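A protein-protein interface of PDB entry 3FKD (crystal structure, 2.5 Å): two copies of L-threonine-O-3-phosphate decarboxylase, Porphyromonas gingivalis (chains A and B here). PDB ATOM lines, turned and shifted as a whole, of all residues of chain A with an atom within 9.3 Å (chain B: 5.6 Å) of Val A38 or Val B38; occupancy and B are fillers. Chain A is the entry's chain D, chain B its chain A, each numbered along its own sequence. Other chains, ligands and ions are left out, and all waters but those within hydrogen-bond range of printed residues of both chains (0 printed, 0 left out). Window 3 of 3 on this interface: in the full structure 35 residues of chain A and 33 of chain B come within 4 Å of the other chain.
OD1 of Asn A42 lies close to OE2 of Glu B34, 3.4 Å away.
Among the printed residues, merely in contact across the chains: Glu A34 with Leu B41, Leu A41 with Val B38, Leu A41 with Glu B34, Ile A44 with Leu B37, Val A38 with Val B38 and Val A38 with Leu B41.
Of the printed residues of chain B, Val A38 touches Val B38 and Leu B41.
Val B38 touches just these residues of chain A: Val A38 and Leu A41.
Printed residues of chain B within 4 Å of Ile A44: Leu B37 (3.9 Å).
Printed residues of chain A within 4 Å of Glu B34: Leu A41 (3.6 Å) and Asn A42 (3.4 Å).
Of the printed residues of chain A, Leu B37 touches Ile A44.
Of the printed residues of chain A, Leu B41 touches Glu A34 (3.6 Å) and Val A38 (3.99 Å).
The nearest residue of chain A that does not touch Val B38 is Glu A34 (6.5 Å).
Of the 17 printed residues of chain A, 5 touch a printed residue of chain B.
Of the 9 printed residues of chain B, 4 touch a printed residue of chain A.
Hydrophobic or aromatic side chains of chain B that line the printed part of chain A: Leu B37, Val B38 and Leu B41.
Among the printed residues, 7 pairs touch across the chains.
Among the printed residues, no Asp or Glu carboxylate lies within 4 Å of a Lys or Arg side-chain nitrogen of the other chain.
Glu A34 touches Leu B41, and with the chains exchanged Leu A41 touches Glu B34.
Val A38 touches its own counterpart, Val B38.
Val A38 touches Leu B41, and with the chains exchanged Leu A41 touches Val B38.
Positions printed for both chains: 33, 34, 35, 36, 37, 38, 39, 40 and 41.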
ATOM      1  N   ASP A  31     -23.847 -12.126 -17.355  1.00  0.00           N
ATOM      2  CA  ASP A  31     -22.946 -11.902 -16.233  1.00  0.00           C
ATOM      3  C   ASP A  31     -23.266 -12.797 -15.056  1.00  0.00           C
ATOM      4  O   ASP A  31     -22.609 -12.688 -14.042  1.00  0.00           O
ATOM      5  CB  ASP A  31     -22.980 -10.430 -15.765  1.00  0.00           C
ATOM      6  CG  ASP A  31     -23.488  -9.461 -16.851  1.00  0.00           C
ATOM      7  OD1 ASP A  31     -24.415  -9.833 -17.629  1.00  0.00           O
ATOM      8  OD2 ASP A  31     -22.959  -8.313 -16.893  1.00  0.00           O
ATOM      9  N   HIS A  32     -24.274 -13.654 -15.150  1.00  0.00           N
ATOM     10  CA  HIS A  32     -24.481 -14.582 -14.044  1.00  0.00           C
ATOM     11  C   HIS A  32     -23.415 -15.672 -13.938  1.00  0.00           C
ATOM     12  O   HIS A  32     -22.977 -16.007 -12.841  1.00  0.00           O
ATOM     13  CB  HIS A  32     -25.903 -15.085 -13.972  1.00  0.00           C
ATOM     14  CG  HIS A  32     -26.877 -13.984 -13.748  1.00  0.00           C
ATOM     15  ND1 HIS A  32     -27.831 -13.631 -14.681  1.00  0.00           N
ATOM     16  CD2 HIS A  32     -26.985 -13.089 -12.735  1.00  0.00           C
ATOM     17  CE1 HIS A  32     -28.519 -12.596 -14.227  1.00  0.00           C
ATOM     18  NE2 HIS A  32     -28.019 -12.242 -13.053  1.00  0.00           N
ATOM     19  N   LEU A  33     -22.935 -16.165 -15.062  1.00  0.00           N
ATOM     20  CA  LEU A  33     -21.713 -16.949 -15.031  1.00  0.00           C
ATOM     21  C   LEU A  33     -20.490 -16.065 -14.765  1.00  0.00           C
ATOM     22  O   LEU A  33     -19.575 -16.471 -14.052  1.00  0.00           O
ATOM     23  CB  LEU A  33     -21.555 -17.717 -16.343  1.00  0.00           C
ATOM     24  CG  LEU A  33     -20.176 -18.269 -16.689  1.00  0.00           C
ATOM     25  CD1 LEU A  33     -19.703 -19.286 -15.628  1.00  0.00           C
ATOM     26  CD2 LEU A  33     -20.217 -18.847 -18.101  1.00  0.00           C
ATOM     27  N   GLU A  34     -20.454 -14.875 -15.336  1.00  0.00           N
ATOM     28  CA  GLU A  34     -19.334 -13.960 -15.067  1.00  0.00           C
ATOM     29  C   GLU A  34     -19.255 -13.384 -13.644  1.00  0.00           C
ATOM     30  O   GLU A  34     -18.149 -13.240 -13.105  1.00  0.00           O
ATOM     31  CB  GLU A  34     -19.212 -12.855 -16.122  1.00  0.00           C
ATOM     32  CG  GLU A  34     -18.595 -13.384 -17.386  1.00  0.00           C
ATOM     33  CD  GLU A  34     -18.589 -12.393 -18.538  1.00  0.00           C
ATOM     34  OE1 GLU A  34     -18.572 -11.160 -18.268  1.00  0.00           O
ATOM     35  OE2 GLU A  34     -18.578 -12.862 -19.711  1.00  0.00           O
ATOM     36  N   LYS A  35     -20.398 -13.082 -13.032  1.00  0.00           N
ATOM     37  CA  LYS A  35     -20.413 -12.695 -11.628  1.00  0.00           C
ATOM     38  C   LYS A  35     -19.781 -13.833 -10.807  1.00  0.00           C
ATOM     39  O   LYS A  35     -18.918 -13.614  -9.959  1.00  0.00           O
ATOM     40  CB  LYS A  35     -21.838 -12.398 -11.131  1.00  0.00           C
ATOM     41  N   HIS A  36     -20.211 -15.051 -11.103  1.00  0.00           N
ATOM     42  CA  HIS A  36     -19.687 -16.221 -10.449  1.00  0.00           C
ATOM     43  C   HIS A  36     -18.185 -16.337 -10.548  1.00  0.00           C
ATOM     44  O   HIS A  36     -17.515 -16.578  -9.549  1.00  0.00           O
ATOM     45  CB  HIS A  36     -20.311 -17.492 -11.009  1.00  0.00           C
ATOM     46  CG  HIS A  36     -20.064 -18.680 -10.143  1.00  0.00           C
ATOM     47  ND1 HIS A  36     -20.545 -18.765  -8.854  1.00  0.00           N
ATOM     48  CD2 HIS A  36     -19.345 -19.805 -10.356  1.00  0.00           C
ATOM     49  CE1 HIS A  36     -20.161 -19.912  -8.321  1.00  0.00           C
ATOM     50  NE2 HIS A  36     -19.423 -20.556  -9.208  1.00  0.00           N
ATOM     51  N   LEU A  37     -17.662 -16.204 -11.758  1.00  0.00           N
ATOM     52  CA  LEU A  37     -16.223 -16.306 -11.954  1.00  0.00           C
ATOM     53  C   LEU A  37     -15.483 -15.196 -11.166  1.00  0.00           C
ATOM     54  O   LEU A  37     -14.437 -15.425 -10.553  1.00  0.00           O
ATOM     55  CB  LEU A  37     -15.906 -16.241 -13.438  1.00  0.00           C
ATOM     56  CG  LEU A  37     -15.492 -17.515 -14.186  1.00  0.00           C
ATOM     57  CD1 LEU A  37     -16.014 -18.877 -13.604  1.00  0.00           C
ATOM     58  CD2 LEU A  37     -15.831 -17.344 -15.682  1.00  0.00           C
ATOM     59  N   VAL A  38     -16.049 -13.995 -11.200  1.00  0.00           N
ATOM     60  CA  VAL A  38     -15.474 -12.852 -10.508  1.00  0.00           C
ATOM     61  C   VAL A  38     -15.482 -13.119  -9.014  1.00  0.00           C
ATOM     62  O   VAL A  38     -14.486 -12.890  -8.334  1.00  0.00           O
ATOM     63  CB  VAL A  38     -16.249 -11.554 -10.802  1.00  0.00           C
ATOM     64  CG1 VAL A  38     -15.895 -10.494  -9.775  1.00  0.00           C
ATOM     65  CG2 VAL A  38     -15.954 -11.087 -12.188  1.00  0.00           C
ATOM     66  N   GLU A  39     -16.590 -13.652  -8.510  1.00  0.00           N
ATOM     67  CA  GLU A  39     -16.627 -14.011  -7.101  1.00  0.00           C
ATOM     68  C   GLU A  39     -15.619 -15.107  -6.735  1.00  0.00           C
ATOM     69  O   GLU A  39     -15.090 -15.073  -5.650  1.00  0.00           O
ATOM     70  CB  GLU A  39     -18.051 -14.338  -6.631  1.00  0.00           C
ATOM     71  CG  GLU A  39     -18.945 -13.123  -6.690  1.00  0.00           C
ATOM     72  CD  GLU A  39     -20.437 -13.435  -6.592  1.00  0.00           C
ATOM     73  OE1 GLU A  39     -21.197 -12.455  -6.438  1.00  0.00           O
ATOM     74  OE2 GLU A  39     -20.851 -14.629  -6.679  1.00  0.00           O
ATOM     75  N   ASN A  40     -15.341 -16.049  -7.643  1.00  0.00           N
ATOM     76  CA  ASN A  40     -14.474 -17.191  -7.330  1.00  0.00           C
ATOM     77  C   ASN A  40     -13.126 -17.132  -8.009  1.00  0.00           C
ATOM     78  O   ASN A  40     -12.490 -18.146  -8.290  1.00  0.00           O
ATOM     79  CB  ASN A  40     -15.172 -18.525  -7.622  1.00  0.00           C
ATOM     80  CG  ASN A  40     -16.423 -18.707  -6.787  1.00  0.00           C
ATOM     81  OD1 ASN A  40     -16.359 -19.161  -5.641  1.00  0.00           O
ATOM     82  ND2 ASN A  40     -17.559 -18.330  -7.341  1.00  0.00           N
ATOM     83  N   LEU A  41     -12.681 -15.916  -8.236  1.00  0.00           N
ATOM     84  CA  LEU A  41     -11.421 -15.688  -8.894  1.00  0.00           C
ATOM     85  C   LEU A  41     -10.221 -16.269  -8.141  1.00  0.00           C
ATOM     86  O   LEU A  41      -9.213 -16.627  -8.764  1.00  0.00           O
ATOM     87  CB  LEU A  41     -11.255 -14.188  -9.163  1.00  0.00           C
ATOM     88  CG  LEU A  41     -10.304 -13.879 -10.326  1.00  0.00           C
ATOM     89  CD1 LEU A  41     -10.460 -14.829 -11.543  1.00  0.00           C
ATOM     90  CD2 LEU A  41     -10.498 -12.448 -10.730  1.00  0.00           C
ATOM     91  N   ASN A  42     -10.320 -16.347  -6.808  1.00  0.00           N
ATOM     92  CA  ASN A  42      -9.244 -16.891  -5.985  1.00  0.00           C
ATOM     93  C   ASN A  42      -8.866 -18.338  -6.351  1.00  0.00           C
ATOM     94  O   ASN A  42      -7.782 -18.790  -6.007  1.00  0.00           O
ATOM     95  CB  ASN A  42      -9.573 -16.813  -4.484  1.00  0.00           C
ATOM     96  CG  ASN A  42      -9.528 -15.387  -3.934  1.00  0.00           C
ATOM     97  OD1 ASN A  42      -9.050 -14.455  -4.604  1.00  0.00           O
ATOM     98  ND2 ASN A  42     -10.048 -15.207  -2.709  1.00  0.00           N
ATOM     99  N   CYS A  43      -9.747 -19.054  -7.049  1.00  0.00           N
ATOM    100  CA  CYS A  43      -9.426 -20.398  -7.506  1.00  0.00           C
ATOM    101  C   CYS A  43      -8.165 -20.436  -8.353  1.00  0.00           C
ATOM    102  O   CYS A  43      -7.600 -21.476  -8.551  1.00  0.00           O
ATOM    103  CB  CYS A  43     -10.616 -21.031  -8.246  1.00  0.00           C
ATOM    104  SG  CYS A  43     -10.836 -20.514  -9.947  1.00  0.00           S
ATOM    105  N   ILE A  44      -7.714 -19.287  -8.842  1.00  0.00           N
ATOM    106  CA  ILE A  44      -6.494 -19.251  -9.646  1.00  0.00           C
ATOM    107  C   ILE A  44      -5.212 -19.279  -8.790  1.00  0.00           C
ATOM    108  O   ILE A  44      -4.107 -19.354  -9.318  1.00  0.00           O
ATOM    109  CB  ILE A  44      -6.463 -18.042 -10.589  1.00  0.00           C
ATOM    110  CG1 ILE A  44      -6.211 -16.747  -9.827  1.00  0.00           C
ATOM    111  CG2 ILE A  44      -7.738 -17.970 -11.405  1.00  0.00           C
ATOM    112  CD1 ILE A  44      -5.867 -15.555 -10.775  1.00  0.00           C
ATOM    113  N   LEU A 231     -10.375 -21.957 -13.603  1.00  0.00           N
ATOM    114  CA  LEU A 231     -11.547 -21.160 -14.011  1.00  0.00           C
ATOM    115  C   LEU A 231     -12.505 -21.955 -14.895  1.00  0.00           C
ATOM    116  O   LEU A 231     -13.714 -21.969 -14.649  1.00  0.00           O
ATOM    117  CB  LEU A 231     -11.130 -19.870 -14.685  1.00  0.00           C
ATOM    118  CG  LEU A 231     -10.785 -18.876 -13.584  1.00  0.00           C
ATOM    119  CD1 LEU A 231     -10.039 -17.648 -14.107  1.00  0.00           C
ATOM    120  CD2 LEU A 231     -12.034 -18.481 -12.745  1.00  0.00           C
ATOM    121  N   GLU A 234     -14.417 -24.383 -12.683  1.00  0.00           N
ATOM    122  CA  GLU A 234     -15.386 -23.565 -11.968  1.00  0.00           C
ATOM    123  C   GLU A 234     -16.547 -23.126 -12.875  1.00  0.00           C
ATOM    124  O   GLU A 234     -17.694 -23.164 -12.475  1.00  0.00           O
ATOM    125  CB  GLU A 234     -14.693 -22.339 -11.357  1.00  0.00           C
ATOM    126  CG  GLU A 234     -15.566 -21.506 -10.468  1.00  0.00           C
ATOM    127  CD  GLU A 234     -16.011 -22.263  -9.219  1.00  0.00           C
ATOM    128  OE1 GLU A 234     -15.221 -23.060  -8.662  1.00  0.00           O
ATOM    129  OE2 GLU A 234     -17.162 -22.057  -8.794  1.00  0.00           O
ATOM    130  N   ALA A 235     -16.238 -22.715 -14.094  1.00  0.00           N
ATOM    131  CA  ALA A 235     -17.266 -22.307 -15.037  1.00  0.00           C
ATOM    132  C   ALA A 235     -18.149 -23.494 -15.435  1.00  0.00           C
ATOM    133  O   ALA A 235     -19.373 -23.384 -15.451  1.00  0.00           O
ATOM    134  CB  ALA A 235     -16.641 -21.651 -16.277  1.00  0.00           C
ATOM    135  N   LEU B  33      -3.468  -7.626 -10.246  1.00  0.00           N
ATOM    136  CA  LEU B  33      -3.607  -8.648 -11.230  1.00  0.00           C
ATOM    137  C   LEU B  33      -5.094  -9.040 -11.311  1.00  0.00           C
ATOM    138  O   LEU B  33      -5.670  -9.127 -12.389  1.00  0.00           O
ATOM    139  CB  LEU B  33      -2.733  -9.853 -10.878  1.00  0.00           C
ATOM    140  CG  LEU B  33      -3.043 -11.132 -11.663  1.00  0.00           C
ATOM    141  CD1 LEU B  33      -2.911 -10.895 -13.149  1.00  0.00           C
ATOM    142  CD2 LEU B  33      -2.142 -12.270 -11.244  1.00  0.00           C
ATOM    143  N   GLU B  34      -5.725  -9.293 -10.179  1.00  0.00           N
ATOM    144  CA  GLU B  34      -7.086  -9.818 -10.201  1.00  0.00           C
ATOM    145  C   GLU B  34      -8.135  -8.816 -10.690  1.00  0.00           C
ATOM    146  O   GLU B  34      -9.056  -9.184 -11.369  1.00  0.00           O
ATOM    147  CB  GLU B  34      -7.461 -10.375  -8.827  1.00  0.00           C
ATOM    148  CG  GLU B  34      -6.748 -11.673  -8.521  1.00  0.00           C
ATOM    149  CD  GLU B  34      -7.184 -12.282  -7.209  1.00  0.00           C
ATOM    150  OE1 GLU B  34      -7.883 -11.569  -6.446  1.00  0.00           O
ATOM    151  OE2 GLU B  34      -6.832 -13.453  -6.952  1.00  0.00           O
ATOM    152  N   LYS B  35      -8.012  -7.560 -10.302  1.00  0.00           N
ATOM    153  CA  LYS B  35      -8.827  -6.529 -10.873  1.00  0.00           C
ATOM    154  C   LYS B  35      -8.666  -6.524 -12.397  1.00  0.00           C
ATOM    155  O   LYS B  35      -9.663  -6.414 -13.117  1.00  0.00           O
ATOM    156  CB  LYS B  35      -8.466  -5.165 -10.274  1.00  0.00           C
ATOM    157  CG  LYS B  35      -9.206  -4.000 -10.917  1.00  0.00           C
ATOM    158  CD  LYS B  35     -10.689  -4.346 -11.094  1.00  0.00           C
ATOM    159  CE  LYS B  35     -11.581  -3.152 -10.749  1.00  0.00           C
ATOM    160  NZ  LYS B  35     -11.217  -2.545  -9.419  1.00  0.00           N
ATOM    161  N   HIS B  36      -7.432  -6.655 -12.884  1.00  0.00           N
ATOM    162  CA  HIS B  36      -7.176  -6.713 -14.332  1.00  0.00           C
ATOM    163  C   HIS B  36      -7.943  -7.839 -15.086  1.00  0.00           C
ATOM    164  O   HIS B  36      -8.503  -7.600 -16.139  1.00  0.00           O
ATOM    165  CB  HIS B  36      -5.666  -6.751 -14.651  1.00  0.00           C
ATOM    166  CG  HIS B  36      -5.357  -6.664 -16.116  1.00  0.00           C
ATOM    167  ND1 HIS B  36      -5.403  -5.476 -16.820  1.00  0.00           N
ATOM    168  CD2 HIS B  36      -5.016  -7.619 -17.016  1.00  0.00           C
ATOM    169  CE1 HIS B  36      -5.094  -5.698 -18.086  1.00  0.00           C
ATOM    170  NE2 HIS B  36      -4.851  -6.990 -18.230  1.00  0.00           N
ATOM    171  N   LEU B  37      -7.981  -9.045 -14.546  1.00  0.00           N
ATOM    172  CA  LEU B  37      -8.765 -10.116 -15.153  1.00  0.00           C
ATOM    173  C   LEU B  37     -10.277  -9.860 -15.141  1.00  0.00           C
ATOM    174  O   LEU B  37     -11.024 -10.343 -16.011  1.00  0.00           O
ATOM    175  CB  LEU B  37      -8.481 -11.441 -14.449  1.00  0.00           C
ATOM    176  CG  LEU B  37      -7.007 -11.819 -14.491  1.00  0.00           C
ATOM    177  CD1 LEU B  37      -6.764 -13.036 -13.561  1.00  0.00           C
ATOM    178  CD2 LEU B  37      -6.434 -11.993 -15.918  1.00  0.00           C
ATOM    179  N   VAL B  38     -10.727  -9.131 -14.127  1.00  0.00           N
ATOM    180  CA  VAL B  38     -12.136  -8.822 -13.977  1.00  0.00           C
ATOM    181  C   VAL B  38     -12.514  -7.850 -15.098  1.00  0.00           C
ATOM    182  O   VAL B  38     -13.579  -7.946 -15.730  1.00  0.00           O
ATOM    183  CB  VAL B  38     -12.398  -8.242 -12.570  1.00  0.00           C
ATOM    184  CG1 VAL B  38     -13.818  -7.749 -12.448  1.00  0.00           C
ATOM    185  CG2 VAL B  38     -12.098  -9.311 -11.508  1.00  0.00           C
ATOM    186  N   GLU B  39     -11.598  -6.934 -15.365  1.00  0.00           N
ATOM    187  CA  GLU B  39     -11.792  -5.958 -16.428  1.00  0.00           C
ATOM    188  C   GLU B  39     -11.803  -6.589 -17.835  1.00  0.00           C
ATOM    189  O   GLU B  39     -12.595  -6.184 -18.702  1.00  0.00           O
ATOM    190  CB  GLU B  39     -10.764  -4.823 -16.291  1.00  0.00           C
ATOM    191  CG  GLU B  39     -11.051  -3.904 -15.089  1.00  0.00           C
ATOM    192  CD  GLU B  39      -9.931  -2.937 -14.781  1.00  0.00           C
ATOM    193  OE1 GLU B  39      -8.928  -2.939 -15.524  1.00  0.00           O
ATOM    194  OE2 GLU B  39     -10.043  -2.182 -13.789  1.00  0.00           O
ATOM    195  N   ASN B  40     -10.941  -7.579 -18.053  1.00  0.00           N
ATOM    196  CA  ASN B  40     -10.841  -8.245 -19.349  1.00  0.00           C
ATOM    197  C   ASN B  40     -11.446  -9.619 -19.371  1.00  0.00           C
ATOM    198  O   ASN B  40     -11.011 -10.489 -20.130  1.00  0.00           O
ATOM    199  CB  ASN B  40      -9.394  -8.304 -19.814  1.00  0.00           C
ATOM    200  CG  ASN B  40      -8.781  -6.926 -19.906  1.00  0.00           C
ATOM    201  OD1 ASN B  40      -8.890  -6.251 -20.944  1.00  0.00           O
ATOM    202  ND2 ASN B  40      -8.162  -6.472 -18.799  1.00  0.00           N
ATOM    203  N   LEU B  41     -12.493  -9.795 -18.577  1.00  0.00           N
ATOM    204  CA  LEU B  41     -13.157 -11.076 -18.483  1.00  0.00           C
ATOM    205  C   LEU B  41     -13.795 -11.571 -19.782  1.00  0.00           C
ATOM    206  O   LEU B  41     -13.922 -12.779 -19.990  1.00  0.00           O
ATOM    207  CB  LEU B  41     -14.160 -11.098 -17.344  1.00  0.00           C
ATOM    208  CG  LEU B  41     -14.416 -12.550 -16.909  1.00  0.00           C
ATOM    209  CD1 LEU B  41     -13.129 -13.298 -16.475  1.00  0.00           C
ATOM    210  CD2 LEU B  41     -15.479 -12.628 -15.833  1.00  0.00           C
